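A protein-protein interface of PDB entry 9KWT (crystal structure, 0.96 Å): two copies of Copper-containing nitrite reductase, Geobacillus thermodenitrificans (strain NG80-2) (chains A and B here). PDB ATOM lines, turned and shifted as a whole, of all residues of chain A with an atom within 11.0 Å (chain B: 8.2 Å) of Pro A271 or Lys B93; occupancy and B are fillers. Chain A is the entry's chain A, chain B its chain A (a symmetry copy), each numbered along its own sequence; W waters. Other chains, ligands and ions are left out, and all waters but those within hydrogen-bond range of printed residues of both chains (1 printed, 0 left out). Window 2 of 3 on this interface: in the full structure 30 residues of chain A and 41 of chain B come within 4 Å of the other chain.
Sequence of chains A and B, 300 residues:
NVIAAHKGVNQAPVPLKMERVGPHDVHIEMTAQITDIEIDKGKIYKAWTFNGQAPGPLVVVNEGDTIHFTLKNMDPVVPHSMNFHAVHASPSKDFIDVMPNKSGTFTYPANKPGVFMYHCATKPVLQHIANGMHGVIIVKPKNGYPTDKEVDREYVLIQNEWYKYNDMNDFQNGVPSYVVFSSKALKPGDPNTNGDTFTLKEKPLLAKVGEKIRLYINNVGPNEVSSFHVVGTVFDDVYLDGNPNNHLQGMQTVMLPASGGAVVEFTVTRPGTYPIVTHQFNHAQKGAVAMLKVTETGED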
ATOM      1  N   LEU A 205      17.645 -18.498   2.388  1.00  0.00           N
ATOM      2  CA  LEU A 205      17.290 -17.560   3.437  1.00  0.00           C
ATOM      3  C   LEU A 205      18.372 -17.608   4.505  1.00  0.00           C
ATOM      4  O   LEU A 205      18.998 -18.647   4.715  1.00  0.00           O
ATOM      5  CB  LEU A 205      15.951 -17.960   4.047  1.00  0.00           C
ATOM      6  CG  LEU A 205      14.765 -17.983   3.084  1.00  0.00           C
ATOM      7  CD1 LEU A 205      13.517 -18.471   3.806  1.00  0.00           C
ATOM      8  CD2 LEU A 205      14.533 -16.614   2.488  1.00  0.00           C
ATOM      9  N   LEU A 206      18.580 -16.494   5.197  1.00  0.00           N
ATOM     10  CA  LEU A 206      19.668 -16.370   6.161  1.00  0.00           C
ATOM     11  C   LEU A 206      19.165 -16.230   7.587  1.00  0.00           C
ATOM     12  O   LEU A 206      18.164 -15.558   7.837  1.00  0.00           O
ATOM     13  CB  LEU A 206      20.553 -15.178   5.815  1.00  0.00           C
ATOM     14  CG  LEU A 206      21.123 -15.198   4.397  1.00  0.00           C
ATOM     15  CD1 LEU A 206      21.941 -13.942   4.170  1.00  0.00           C
ATOM     16  CD2 LEU A 206      21.992 -16.421   4.169  1.00  0.00           C
ATOM     17  N   ALA A 207      19.886 -16.825   8.528  1.00  0.00           N
ATOM     18  CA  ALA A 207      19.588 -16.638   9.938  1.00  0.00           C
ATOM     19  C   ALA A 207      20.853 -16.853  10.757  1.00  0.00           C
ATOM     20  O   ALA A 207      21.901 -17.244  10.233  1.00  0.00           O
ATOM     21  CB  ALA A 207      18.483 -17.576  10.413  1.00  0.00           C
ATOM     22  N   LYS A 208      20.727 -16.629  12.059  1.00  0.00           N
ATOM     23  CA  LYS A 208      21.844 -16.701  12.992  1.00  0.00           C
ATOM     24  C   LYS A 208      21.612 -17.811  14.007  1.00  0.00           C
ATOM     25  O   LYS A 208      20.485 -18.026  14.464  1.00  0.00           O
ATOM     26  CB  LYS A 208      21.990 -15.366  13.727  1.00  0.00           C
ATOM     27  CG  LYS A 208      23.145 -15.272  14.691  1.00  0.00           C
ATOM     28  CD  LYS A 208      23.276 -13.847  15.215  1.00  0.00           C
ATOM     29  CE  LYS A 208      24.324 -13.749  16.306  1.00  0.00           C
ATOM     30  NZ  LYS A 208      23.725 -13.995  17.638  1.00  0.00           N
ATOM     31  N   VAL A 209      22.703 -18.482  14.386  1.00  0.00           N
ATOM     32  CA  VAL A 209      22.633 -19.580  15.345  1.00  0.00           C
ATOM     33  C   VAL A 209      21.873 -19.138  16.585  1.00  0.00           C
ATOM     34  O   VAL A 209      22.151 -18.080  17.168  1.00  0.00           O
ATOM     35  CB  VAL A 209      24.044 -20.071  15.712  1.00  0.00           C
ATOM     36  CG1 VAL A 209      23.987 -21.107  16.840  1.00  0.00           C
ATOM     37  CG2 VAL A 209      24.735 -20.656  14.513  1.00  0.00           C
ATOM     38  N   GLY A 210      20.945 -19.990  17.025  1.00  0.00           N
ATOM     39  CA  GLY A 210      20.181 -19.760  18.229  1.00  0.00           C
ATOM     40  C   GLY A 210      18.879 -19.024  18.029  1.00  0.00           C
ATOM     41  O   GLY A 210      18.075 -18.952  18.967  1.00  0.00           O
ATOM     42  N   GLU A 211      18.638 -18.478  16.845  1.00  0.00           N
ATOM     43  CA  GLU A 211      17.453 -17.669  16.635  1.00  0.00           C
ATOM     44  C   GLU A 211      16.182 -18.503  16.573  1.00  0.00           C
ATOM     45  O   GLU A 211      16.165 -19.658  16.121  1.00  0.00           O
ATOM     46  CB  GLU A 211      17.558 -16.867  15.340  1.00  0.00           C
ATOM     47  CG  GLU A 211      18.482 -15.677  15.463  1.00  0.00           C
ATOM     48  CD  GLU A 211      18.529 -14.807  14.227  1.00  0.00           C
ATOM     49  OE1 GLU A 211      18.326 -15.333  13.109  1.00  0.00           O
ATOM     50  OE2 GLU A 211      18.821 -13.600  14.387  1.00  0.00           O
ATOM     51  N   VAL A 231      13.724 -29.212   8.212  1.00  0.00           N
ATOM     52  CA  VAL A 231      14.668 -30.237   8.629  1.00  0.00           C
ATOM     53  C   VAL A 231      15.542 -29.722   9.763  1.00  0.00           C
ATOM     54  O   VAL A 231      16.025 -28.589   9.729  1.00  0.00           O
ATOM     55  CB  VAL A 231      15.516 -30.646   7.413  1.00  0.00           C
ATOM     56  CG1 VAL A 231      16.551 -31.689   7.779  1.00  0.00           C
ATOM     57  CG2 VAL A 231      14.634 -31.161   6.300  1.00  0.00           C
ATOM     58  N   GLY A 232      15.776 -30.570  10.774  1.00  0.00           N
ATOM     59  CA  GLY A 232      16.690 -30.231  11.849  1.00  0.00           C
ATOM     60  C   GLY A 232      16.093 -29.428  12.977  1.00  0.00           C
ATOM     61  O   GLY A 232      16.818 -29.020  13.889  1.00  0.00           O
ATOM     62  N   THR A 267      13.227 -22.984  16.327  1.00  0.00           N
ATOM     63  CA  THR A 267      14.540 -22.556  16.762  1.00  0.00           C
ATOM     64  C   THR A 267      15.604 -23.328  15.994  1.00  0.00           C
ATOM     65  O   THR A 267      15.501 -24.549  15.832  1.00  0.00           O
ATOM     66  CB  THR A 267      14.669 -22.777  18.273  1.00  0.00           C
ATOM     67  OG1 THR A 267      13.596 -22.092  18.944  1.00  0.00           O
ATOM     68  CG2 THR A 267      15.998 -22.266  18.787  1.00  0.00           C
ATOM     69  N   VAL A 268      16.629 -22.616  15.524  1.00  0.00           N
ATOM     70  CA  VAL A 268      17.767 -23.220  14.840  1.00  0.00           C
ATOM     71  C   VAL A 268      18.950 -23.174  15.801  1.00  0.00           C
ATOM     72  O   VAL A 268      19.420 -22.099  16.188  1.00  0.00           O
ATOM     73  CB  VAL A 268      18.067 -22.556  13.485  1.00  0.00           C
ATOM     74  CG1 VAL A 268      16.993 -22.933  12.477  1.00  0.00           C
ATOM     75  CG2 VAL A 268      18.202 -21.031  13.589  1.00  0.00           C
ATOM     76  N   THR A 269      19.416 -24.339  16.226  1.00  0.00           N
ATOM     77  CA  THR A 269      20.330 -24.400  17.354  1.00  0.00           C
ATOM     78  C   THR A 269      21.799 -24.468  16.970  1.00  0.00           C
ATOM     79  O   THR A 269      22.648 -24.241  17.839  1.00  0.00           O
ATOM     80  CB  THR A 269      20.023 -25.623  18.218  1.00  0.00           C
ATOM     81  OG1 THR A 269      20.223 -26.801  17.431  1.00  0.00           O
ATOM     82  CG2 THR A 269      18.597 -25.588  18.767  1.00  0.00           C
ATOM     83  N   ARG A 270      22.119 -24.788  15.723  1.00  0.00           N
ATOM     84  CA  ARG A 270      23.478 -25.076  15.296  1.00  0.00           C
ATOM     85  C   ARG A 270      23.736 -24.439  13.942  1.00  0.00           C
ATOM     86  O   ARG A 270      22.813 -24.272  13.137  1.00  0.00           O
ATOM     87  CB  ARG A 270      23.726 -26.590  15.200  1.00  0.00           C
ATOM     88  CG  ARG A 270      23.724 -27.273  16.548  1.00  0.00           C
ATOM     89  CD  ARG A 270      23.865 -28.767  16.424  1.00  0.00           C
ATOM     90  NE  ARG A 270      23.882 -29.367  17.748  1.00  0.00           N
ATOM     91  CZ  ARG A 270      23.960 -30.664  17.992  1.00  0.00           C
ATOM     92  NH1 ARG A 270      24.046 -31.549  17.017  1.00  0.00           N
ATOM     93  NH2 ARG A 270      23.953 -31.081  19.251  1.00  0.00           N
ATOM     94  N   PRO A 271      24.981 -24.080  13.659  1.00  0.00           N
ATOM     95  CA  PRO A 271      25.299 -23.584  12.320  1.00  0.00           C
ATOM     96  C   PRO A 271      25.121 -24.673  11.276  1.00  0.00           C
ATOM     97  O   PRO A 271      25.404 -25.845  11.526  1.00  0.00           O
ATOM     98  CB  PRO A 271      26.768 -23.160  12.442  1.00  0.00           C
ATOM     99  CG  PRO A 271      27.316 -24.051  13.506  1.00  0.00           C
ATOM    100  CD  PRO A 271      26.191 -24.236  14.494  1.00  0.00           C
ATOM    101  N   GLY A 272      24.673 -24.273  10.103  1.00  0.00           N
ATOM    102  CA  GLY A 272      24.530 -25.195   8.995  1.00  0.00           C
ATOM    103  C   GLY A 272      23.433 -24.736   8.060  1.00  0.00           C
ATOM    104  O   GLY A 272      22.842 -23.673   8.229  1.00  0.00           O
ATOM    105  N   THR A 273      23.169 -25.570   7.062  1.00  0.00           N
ATOM    106  CA  THR A 273      22.087 -25.331   6.120  1.00  0.00           C
ATOM    107  C   THR A 273      20.958 -26.307   6.394  1.00  0.00           C
ATOM    108  O   THR A 273      21.185 -27.516   6.526  1.00  0.00           O
ATOM    109  CB  THR A 273      22.579 -25.384   4.675  1.00  0.00           C
ATOM    110  OG1 THR A 273      23.590 -24.384   4.497  1.00  0.00           O
ATOM    111  CG2 THR A 273      21.448 -25.123   3.706  1.00  0.00           C
ATOM    112  N   TYR A 274      19.760 -25.748   6.528  1.00  0.00           N
ATOM    113  CA  TYR A 274      18.555 -26.454   6.937  1.00  0.00           C
ATOM    114  C   TYR A 274      17.581 -26.483   5.769  1.00  0.00           C
ATOM    115  O   TYR A 274      17.026 -25.435   5.411  1.00  0.00           O
ATOM    116  CB  TYR A 274      17.893 -25.741   8.117  1.00  0.00           C
ATOM    117  CG  TYR A 274      18.652 -25.751   9.427  1.00  0.00           C
ATOM    118  CD1 TYR A 274      19.874 -25.115   9.568  1.00  0.00           C
ATOM    119  CD2 TYR A 274      18.119 -26.378  10.540  1.00  0.00           C
ATOM    120  CE1 TYR A 274      20.544 -25.129  10.776  1.00  0.00           C
ATOM    121  CE2 TYR A 274      18.778 -26.386  11.747  1.00  0.00           C
ATOM    122  CZ  TYR A 274      19.993 -25.759  11.863  1.00  0.00           C
ATOM    123  OH  TYR A 274      20.635 -25.792  13.087  1.00  0.00           O
ATOM    124  N   PRO A 275      17.301 -27.640   5.177  1.00  0.00           N
ATOM    125  CA  PRO A 275      16.269 -27.692   4.141  1.00  0.00           C
ATOM    126  C   PRO A 275      14.882 -27.440   4.711  1.00  0.00           C
ATOM    127  O   PRO A 275      14.572 -27.787   5.856  1.00  0.00           O
ATOM    128  CB  PRO A 275      16.401 -29.114   3.575  1.00  0.00           C
ATOM    129  CG  PRO A 275      17.821 -29.530   3.922  1.00  0.00           C
ATOM    130  CD  PRO A 275      18.067 -28.894   5.258  1.00  0.00           C
ATOM    131  N   LEU A 292      17.634 -22.770   4.347  1.00  0.00           N
ATOM    132  CA  LEU A 292      17.890 -21.754   5.361  1.00  0.00           C
ATOM    133  C   LEU A 292      19.317 -21.945   5.859  1.00  0.00           C
ATOM    134  O   LEU A 292      19.646 -22.989   6.432  1.00  0.00           O
ATOM    135  CB  LEU A 292      16.888 -21.924   6.504  1.00  0.00           C
ATOM    136  CG  LEU A 292      17.074 -21.025   7.722  1.00  0.00           C
ATOM    137  CD1 LEU A 292      16.830 -19.558   7.380  1.00  0.00           C
ATOM    138  CD2 LEU A 292      16.166 -21.469   8.847  1.00  0.00           C
ATOM    139  N   LYS A 293      20.169 -20.953   5.620  1.00  0.00           N
ATOM    140  CA  LYS A 293      21.572 -21.003   5.989  1.00  0.00           C
ATOM    141  C   LYS A 293      21.759 -20.235   7.288  1.00  0.00           C
ATOM    142  O   LYS A 293      21.482 -19.035   7.354  1.00  0.00           O
ATOM    143  CB  LYS A 293      22.439 -20.419   4.877  1.00  0.00           C
ATOM    144  CG  LYS A 293      23.916 -20.489   5.179  1.00  0.00           C
ATOM    145  CD  LYS A 293      24.740 -19.929   4.039  1.00  0.00           C
ATOM    146  CE  LYS A 293      26.217 -20.054   4.314  1.00  0.00           C
ATOM    147  NZ  LYS A 293      26.968 -19.082   3.489  1.00  0.00           N
ATOM    148  N   VAL A 294      22.203 -20.951   8.308  1.00  0.00           N
ATOM    149  CA  VAL A 294      22.311 -20.458   9.673  1.00  0.00           C
ATOM    150  C   VAL A 294      23.790 -20.332  10.001  1.00  0.00           C
ATOM    151  O   VAL A 294      24.534 -21.317   9.971  1.00  0.00           O
ATOM    152  CB  VAL A 294      21.608 -21.417  10.642  1.00  0.00           C
ATOM    153  CG1 VAL A 294      21.717 -20.929  12.071  1.00  0.00           C
ATOM    154  CG2 VAL A 294      20.153 -21.611  10.243  1.00  0.00           C
ATOM    155  N   THR A 295      24.223 -19.117  10.295  1.00  0.00           N
ATOM    156  CA  THR A 295      25.625 -18.834  10.549  1.00  0.00           C
ATOM    157  C   THR A 295      25.797 -18.216  11.926  1.00  0.00           C
ATOM    158  O   THR A 295      24.861 -17.744  12.564  1.00  0.00           O
ATOM    159  CB  THR A 295      26.201 -17.899   9.480  1.00  0.00           C
ATOM    160  OG1 THR A 295      25.504 -16.656   9.528  1.00  0.00           O
ATOM    161  CG2 THR A 295      26.068 -18.503   8.100  1.00  0.00           C
ATOM    162  N   GLU A 296      27.043 -18.179  12.375  1.00  0.00           N
ATOM    163  CA  GLU A 296      27.314 -17.560  13.666  1.00  0.00           C
ATOM    164  C   GLU A 296      26.947 -16.072  13.675  1.00  0.00           C
ATOM    165  O   GLU A 296      26.592 -15.539  14.731  1.00  0.00           O
ATOM    166  CB  GLU A 296      28.770 -17.800  14.069  1.00  0.00           C
ATOM    167  CG  GLU A 296      29.100 -19.277  14.360  1.00  0.00           C
ATOM    168  CD  GLU A 296      28.317 -19.881  15.529  1.00  0.00           C
ATOM    169  OE1 GLU A 296      27.755 -19.123  16.346  1.00  0.00           O
ATOM    170  OE2 GLU A 296      28.273 -21.128  15.635  1.00  0.00           O
ATOM    171  N   THR A 297      26.981 -15.394  12.518  1.00  0.00           N
ATOM    172  CA  THR A 297      26.652 -13.967  12.445  1.00  0.00           C
ATOM    173  C   THR A 297      25.282 -13.659  11.850  1.00  0.00           C
ATOM    174  O   THR A 297      24.716 -12.609  12.167  1.00  0.00           O
ATOM    175  CB  THR A 297      27.699 -13.193  11.625  1.00  0.00           C
ATOM    176  OG1 THR A 297      27.654 -13.612  10.253  1.00  0.00           O
ATOM    177  CG2 THR A 297      29.104 -13.396  12.180  1.00  0.00           C
ATOM    178  N   GLY A 298      24.732 -14.528  11.002  1.00  0.00           N
ATOM    179  CA  GLY A 298      23.500 -14.236  10.287  1.00  0.00           C
ATOM    180  C   GLY A 298      23.692 -13.633   8.920  1.00  0.00           C
ATOM    181  O   GLY A 298      22.698 -13.361   8.235  1.00  0.00           O
ATOM    182  N   GLU A 299      24.931 -13.394   8.518  1.00  0.00           N
ATOM    183  CA  GLU A 299      25.274 -12.913   7.195  1.00  0.00           C
ATOM    184  C   GLU A 299      25.954 -14.054   6.449  1.00  0.00           C
ATOM    185  O   GLU A 299      26.502 -14.978   7.057  1.00  0.00           O
ATOM    186  CB  GLU A 299      26.222 -11.712   7.309  1.00  0.00           C
ATOM    187  CG  GLU A 299      25.649 -10.544   8.128  1.00  0.00           C
ATOM    188  CD  GLU A 299      25.035  -9.441   7.283  1.00  0.00           C
ATOM    189  OE1 GLU A 299      25.424  -9.289   6.107  1.00  0.00           O
ATOM    190  OE2 GLU A 299      24.159  -8.717   7.803  1.00  0.00           O
ATOM    191  N   ALA B  89      19.138 -30.329  15.244  1.00  0.00           N
ATOM    192  CA  ALA B  89      20.446 -30.674  14.708  1.00  0.00           C
ATOM    193  C   ALA B  89      20.756 -29.783  13.519  1.00  0.00           C
ATOM    194  O   ALA B  89      19.856 -29.205  12.916  1.00  0.00           O
ATOM    195  CB  ALA B  89      20.478 -32.144  14.283  1.00  0.00           C
ATOM    196  N   SER B  90      22.042 -29.718  13.167  1.00  0.00           N
ATOM    197  CA  SER B  90      22.473 -29.061  11.941  1.00  0.00           C
ATOM    198  C   SER B  90      22.381 -30.073  10.813  1.00  0.00           C
ATOM    199  O   SER B  90      23.165 -31.025  10.798  1.00  0.00           O
ATOM    200  CB  SER B  90      23.911 -28.609  12.068  1.00  0.00           C
ATOM    201  OG  SER B  90      24.398 -28.273  10.781  1.00  0.00           O
ATOM    202  N   PRO B  91      21.477 -29.926   9.845  1.00  0.00           N
ATOM    203  CA  PRO B  91      21.356 -31.013   8.857  1.00  0.00           C
ATOM    204  C   PRO B  91      22.629 -31.245   8.070  1.00  0.00           C
ATOM    205  O   PRO B  91      22.968 -32.394   7.759  1.00  0.00           O
ATOM    206  CB  PRO B  91      20.169 -30.561   8.000  1.00  0.00           C
ATOM    207  CG  PRO B  91      19.338 -29.764   8.972  1.00  0.00           C
ATOM    208  CD  PRO B  91      20.370 -28.965   9.726  1.00  0.00           C
ATOM    209  N   SER B  92      23.347 -30.176   7.740  1.00  0.00           N
ATOM    210  CA  SER B  92      24.553 -30.267   6.924  1.00  0.00           C
ATOM    211  C   SER B  92      25.784 -30.733   7.693  1.00  0.00           C
ATOM    212  O   SER B  92      26.825 -30.947   7.071  1.00  0.00           O
ATOM    213  CB  SER B  92      24.817 -28.925   6.253  1.00  0.00           C
ATOM    214  OG  SER B  92      24.870 -27.889   7.212  1.00  0.00           O
ATOM    215  N   LYS B  93      25.691 -30.895   9.009  1.00  0.00           N
ATOM    216  CA  LYS B  93      26.766 -31.470   9.804  1.00  0.00           C
ATOM    217  C   LYS B  93      26.380 -32.788  10.460  1.00  0.00           C
ATOM    218  O   LYS B  93      27.236 -33.663  10.625  1.00  0.00           O
ATOM    219  CB  LYS B  93      27.197 -30.485  10.905  1.00  0.00           C
ATOM    220  CG  LYS B  93      27.777 -29.186  10.362  1.00  0.00           C
ATOM    221  CD  LYS B  93      28.025 -28.136  11.450  1.00  0.00           C
ATOM    222  CE  LYS B  93      29.220 -28.478  12.329  1.00  0.00           C
ATOM    223  NZ  LYS B  93      29.466 -27.430  13.371  1.00  0.00           N
ATOM    224  N   ASP B  94      25.115 -32.944  10.849  1.00  0.00           N
ATOM    225  CA  ASP B  94      24.684 -34.033  11.704  1.00  0.00           C
ATOM    226  C   ASP B  94      23.859 -35.096  10.991  1.00  0.00           C
ATOM    227  O   ASP B  94      23.687 -36.182  11.552  1.00  0.00           O
ATOM    228  CB  ASP B  94      23.844 -33.481  12.864  1.00  0.00           C
ATOM    229  CG  ASP B  94      24.592 -32.504  13.743  1.00  0.00           C
ATOM    230  OD1 ASP B  94      25.799 -32.715  13.970  1.00  0.00           O
ATOM    231  OD2 ASP B  94      23.951 -31.550  14.238  1.00  0.00           O
ATOM    232  N   PHE B  95      23.323 -34.797   9.800  1.00  0.00           N
ATOM    233  CA  PHE B  95      22.524 -35.731   9.014  1.00  0.00           C
ATOM    234  C   PHE B  95      23.261 -36.119   7.729  1.00  0.00           C
ATOM    235  O   PHE B  95      22.643 -36.447   6.715  1.00  0.00           O
ATOM    236  CB  PHE B  95      21.143 -35.166   8.657  1.00  0.00           C
ATOM    237  CG  PHE B  95      20.211 -34.858   9.818  1.00  0.00           C
ATOM    238  CD1 PHE B  95      20.394 -35.312  11.116  1.00  0.00           C
ATOM    239  CD2 PHE B  95      19.068 -34.123   9.547  1.00  0.00           C
ATOM    240  CE1 PHE B  95      19.459 -35.023  12.116  1.00  0.00           C
ATOM    241  CE2 PHE B  95      18.135 -33.847  10.527  1.00  0.00           C
ATOM    242  CZ  PHE B  95      18.322 -34.295  11.810  1.00  0.00           C
ATOM    243  N   ILE B  96      24.590 -36.121   7.771  1.00  0.00           N
ATOM    244  CA  ILE B  96      25.435 -36.341   6.606  1.00  0.00           C
ATOM    245  C   ILE B  96      25.659 -37.808   6.284  1.00  0.00           C
ATOM    246  O   ILE B  96      25.360 -38.710   7.074  1.00  0.00           O
ATOM    247  CB  ILE B  96      26.761 -35.572   6.739  1.00  0.00           C
ATOM    248  CG1 ILE B  96      27.607 -36.151   7.875  1.00  0.00           C
ATOM    249  CG2 ILE B  96      26.492 -34.075   6.872  1.00  0.00           C
ATOM    250  CD1 ILE B  96      28.999 -35.554   7.965  1.00  0.00           C
ATOM    251  N   ASP B  97      26.195 -38.042   5.097  1.00  0.00           N
ATOM    252  CA  ASP B  97      26.342 -39.391   4.589  1.00  0.00           C
ATOM    253  C   ASP B  97      27.434 -40.170   5.309  1.00  0.00           C
ATOM    254  O   ASP B  97      28.468 -39.633   5.723  1.00  0.00           O
ATOM    255  CB  ASP B  97      26.668 -39.346   3.100  1.00  0.00           C
ATOM    256  CG  ASP B  97      25.486 -38.950   2.242  1.00  0.00           C
ATOM    257  OD1 ASP B  97      24.344 -38.941   2.742  1.00  0.00           O
ATOM    258  OD2 ASP B  97      25.707 -38.590   1.069  1.00  0.00           O
ATOM    259  N   THR B 105      29.047 -41.312  13.634  1.00  0.00           N
ATOM    260  CA  THR B 105      28.365 -41.032  14.894  1.00  0.00           C
ATOM    261  C   THR B 105      28.007 -39.554  14.966  1.00  0.00           C
ATOM    262  O   THR B 105      28.827 -38.689  14.659  1.00  0.00           O
ATOM    263  CB  THR B 105      29.204 -41.453  16.110  1.00  0.00           C
ATOM    264  OG1 THR B 105      29.461 -42.864  16.056  1.00  0.00           O
ATOM    265  CG2 THR B 105      28.476 -41.139  17.427  1.00  0.00           C
ATOM    266  N   PHE B 106      26.779 -39.293  15.410  1.00  0.00           N
ATOM    267  CA  PHE B 106      26.162 -37.973  15.416  1.00  0.00           C
ATOM    268  C   PHE B 106      25.360 -37.830  16.699  1.00  0.00           C
ATOM    269  O   PHE B 106      24.639 -38.754  17.085  1.00  0.00           O
ATOM    270  CB  PHE B 106      25.224 -37.831  14.207  1.00  0.00           C
ATOM    271  CG  PHE B 106      25.893 -38.176  12.918  1.00  0.00           C
ATOM    272  CD1 PHE B 106      26.771 -37.287  12.332  1.00  0.00           C
ATOM    273  CD2 PHE B 106      25.700 -39.416  12.335  1.00  0.00           C
ATOM    274  CE1 PHE B 106      27.428 -37.619  11.171  1.00  0.00           C
ATOM    275  CE2 PHE B 106      26.345 -39.751  11.171  1.00  0.00           C
ATOM    276  CZ  PHE B 106      27.205 -38.855  10.584  1.00  0.00           C
ATOM    277  N   THR B 107      25.470 -36.677  17.353  1.00  0.00           N
ATOM    278  CA  THR B 107      24.832 -36.470  18.646  1.00  0.00           C
ATOM    279  C   THR B 107      23.894 -35.272  18.588  1.00  0.00           C
ATOM    280  O   THR B 107      24.242 -34.222  18.038  1.00  0.00           O
ATOM    281  CB  THR B 107      25.888 -36.297  19.746  1.00  0.00           C
ATOM    282  OG1 THR B 107      26.672 -37.497  19.857  1.00  0.00           O
ATOM    283  CG2 THR B 107      25.225 -36.006  21.060  1.00  0.00           C
ATOM    284  N   TYR B 108      22.696 -35.430  19.149  1.00  0.00           N
ATOM    285  CA  TYR B 108      21.707 -34.363  19.092  1.00  0.00           C
ATOM    286  C   TYR B 108      20.600 -34.624  20.104  1.00  0.00           C
ATOM    287  O   TYR B 108      20.278 -35.787  20.400  1.00  0.00           O
ATOM    288  CB  TYR B 108      21.114 -34.187  17.672  1.00  0.00           C
ATOM    289  CG  TYR B 108      21.177 -35.423  16.792  1.00  0.00           C
ATOM    290  CD1 TYR B 108      20.636 -36.639  17.206  1.00  0.00           C
ATOM    291  CD2 TYR B 108      21.780 -35.376  15.547  1.00  0.00           C
ATOM    292  CE1 TYR B 108      20.700 -37.754  16.404  1.00  0.00           C
ATOM    293  CE2 TYR B 108      21.843 -36.489  14.725  1.00  0.00           C
ATOM    294  CZ  TYR B 108      21.298 -37.683  15.165  1.00  0.00           C
ATOM    295  OH  TYR B 108      21.348 -38.816  14.403  1.00  0.00           O
HETATM  296  O   HOH W   1      24.161 -33.033  21.326  1.00  0.00           O
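No position is printed for both chains. Of the 18 pairs that touch across the chains among the printed residues, none has its exchanged pair printed and touching as well.
Among the printed residues, merely in contact across the chains: Val A231 with Pro B91, Val A231 with Phe B95, Gly A232 with Pro B91, Arg A270 with Ser B90, Arg A270 with Tyr B108, Pro A271 with Lys B93, Gly A272 with Ser B90, Gly A272 with Ser B92, Thr A273 with Pro B91, Tyr A274 with Ala B89, Tyr A274 with Ser B90, Tyr A274 with Pro B91 and Pro A275 with Pro B91.
O of Gly A232 is in hydrogen-bond range of N of Ala B89, at 3.0 Å. OG of Ser B92 sits at hydrogen-bond distance from N of Thr A273, 2.9 Å away. The guanidinium group of Arg A270 lies within hydrogen-bond range of the backbone carbonyl oxygen of Thr B107 (2.9 Å). The side-chain hydroxyl (OG) of Ser B90 is in hydrogen-bond range of the backbone carbonyl oxygen (O) of Pro A271 (2.7 Å). The side-chain carboxylate (OD2) of Asp B94 is in salt-bridge range of the guanidinium group (NH1) of Arg A270, 2.8 Å away.
Water W1 lies within hydrogen-bond range of the guanidinium group of Arg A270 (2.9 Å) and the backbone carbonyl oxygen of Thr B107 (3.5 Å).
Hydrophobic or aromatic side chains of chain B within 4 Å of the printed part of chain A: Pro B91, Phe B95 and Tyr B108. Hydrophobic or aromatic side chains of chain A that line the printed part of chain B: Val A231, Tyr A274 and Pro A275. Among the printed residues, 18 pairs touch across the chains. Among the printed residues, Asp or Glu carboxylates within 4 Å of a Lys or Arg side-chain nitrogen of the other chain: Arg A270 with Asp B94 (2.8 Å).
Of the printed residues of chain B, Pro A271 touches Ser B90 and Lys B93. Printed residues of chain A within 4 Å of Lys B93: Pro A271. Of the printed residues of chain B, Gly A272 touches Ser B90 and Ser B92. Ser B90 touches just these residues of chain A: Arg A270 (3.7 Å), Pro A271 (2.7 Å), Gly A272 (3.6 Å) and Tyr A274 (3.9 Å). Of chain A, only Val A231, Gly A232, Thr A273, Tyr A274 and Pro A275 come within 4 Å of Pro B91. Of chain A, only Gly A272 and Thr A273 come within 4 Å of Ser B92. Of the printed residues of chain B, Pro A275 touches Pro B91 (3.8 Å). Of the printed residues of chain A, Thr B107 touches Arg A270. Of the printed residues of chain B, Val A231 touches Pro B91 (3.6 Å) and Phe B95 (3.8 Å). Ala A207 touches none of the printed residues of chain B. Leu A205 touches none of the printed residues of chain B. The nearest printed residue of chain B that does not touch Pro A271 is Ser B92 (4.8 Å). The nearest printed residue of chain A that does not touch Lys B93 is Gly A272 (5.2 Å).
O of Arg A270 is in hydrogen-bond range of OH of Tyr A274, at 2.7 Å. The backbone NH (N) of Tyr A274 lies within hydrogen-bond range of the backbone carbonyl oxygen (O) of Leu A292 (2.8 Å). The backbone NH (N) of Val A231 lies within hydrogen-bond range of the backbone carbonyl oxygen (O) of Pro A275 (2.9 Å). The backbone NH (N) of Ser B90 lies within hydrogen-bond range of the side-chain carboxylate (OD2) of Asp B94 (2.9 Å). OG of Ser B90 sits at hydrogen-bond distance from N of Lys B93 (3.4 Å). The backbone carbonyl oxygen of Gly A272 sits at hydrogen-bond distance from the backbone NH of Val A294.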
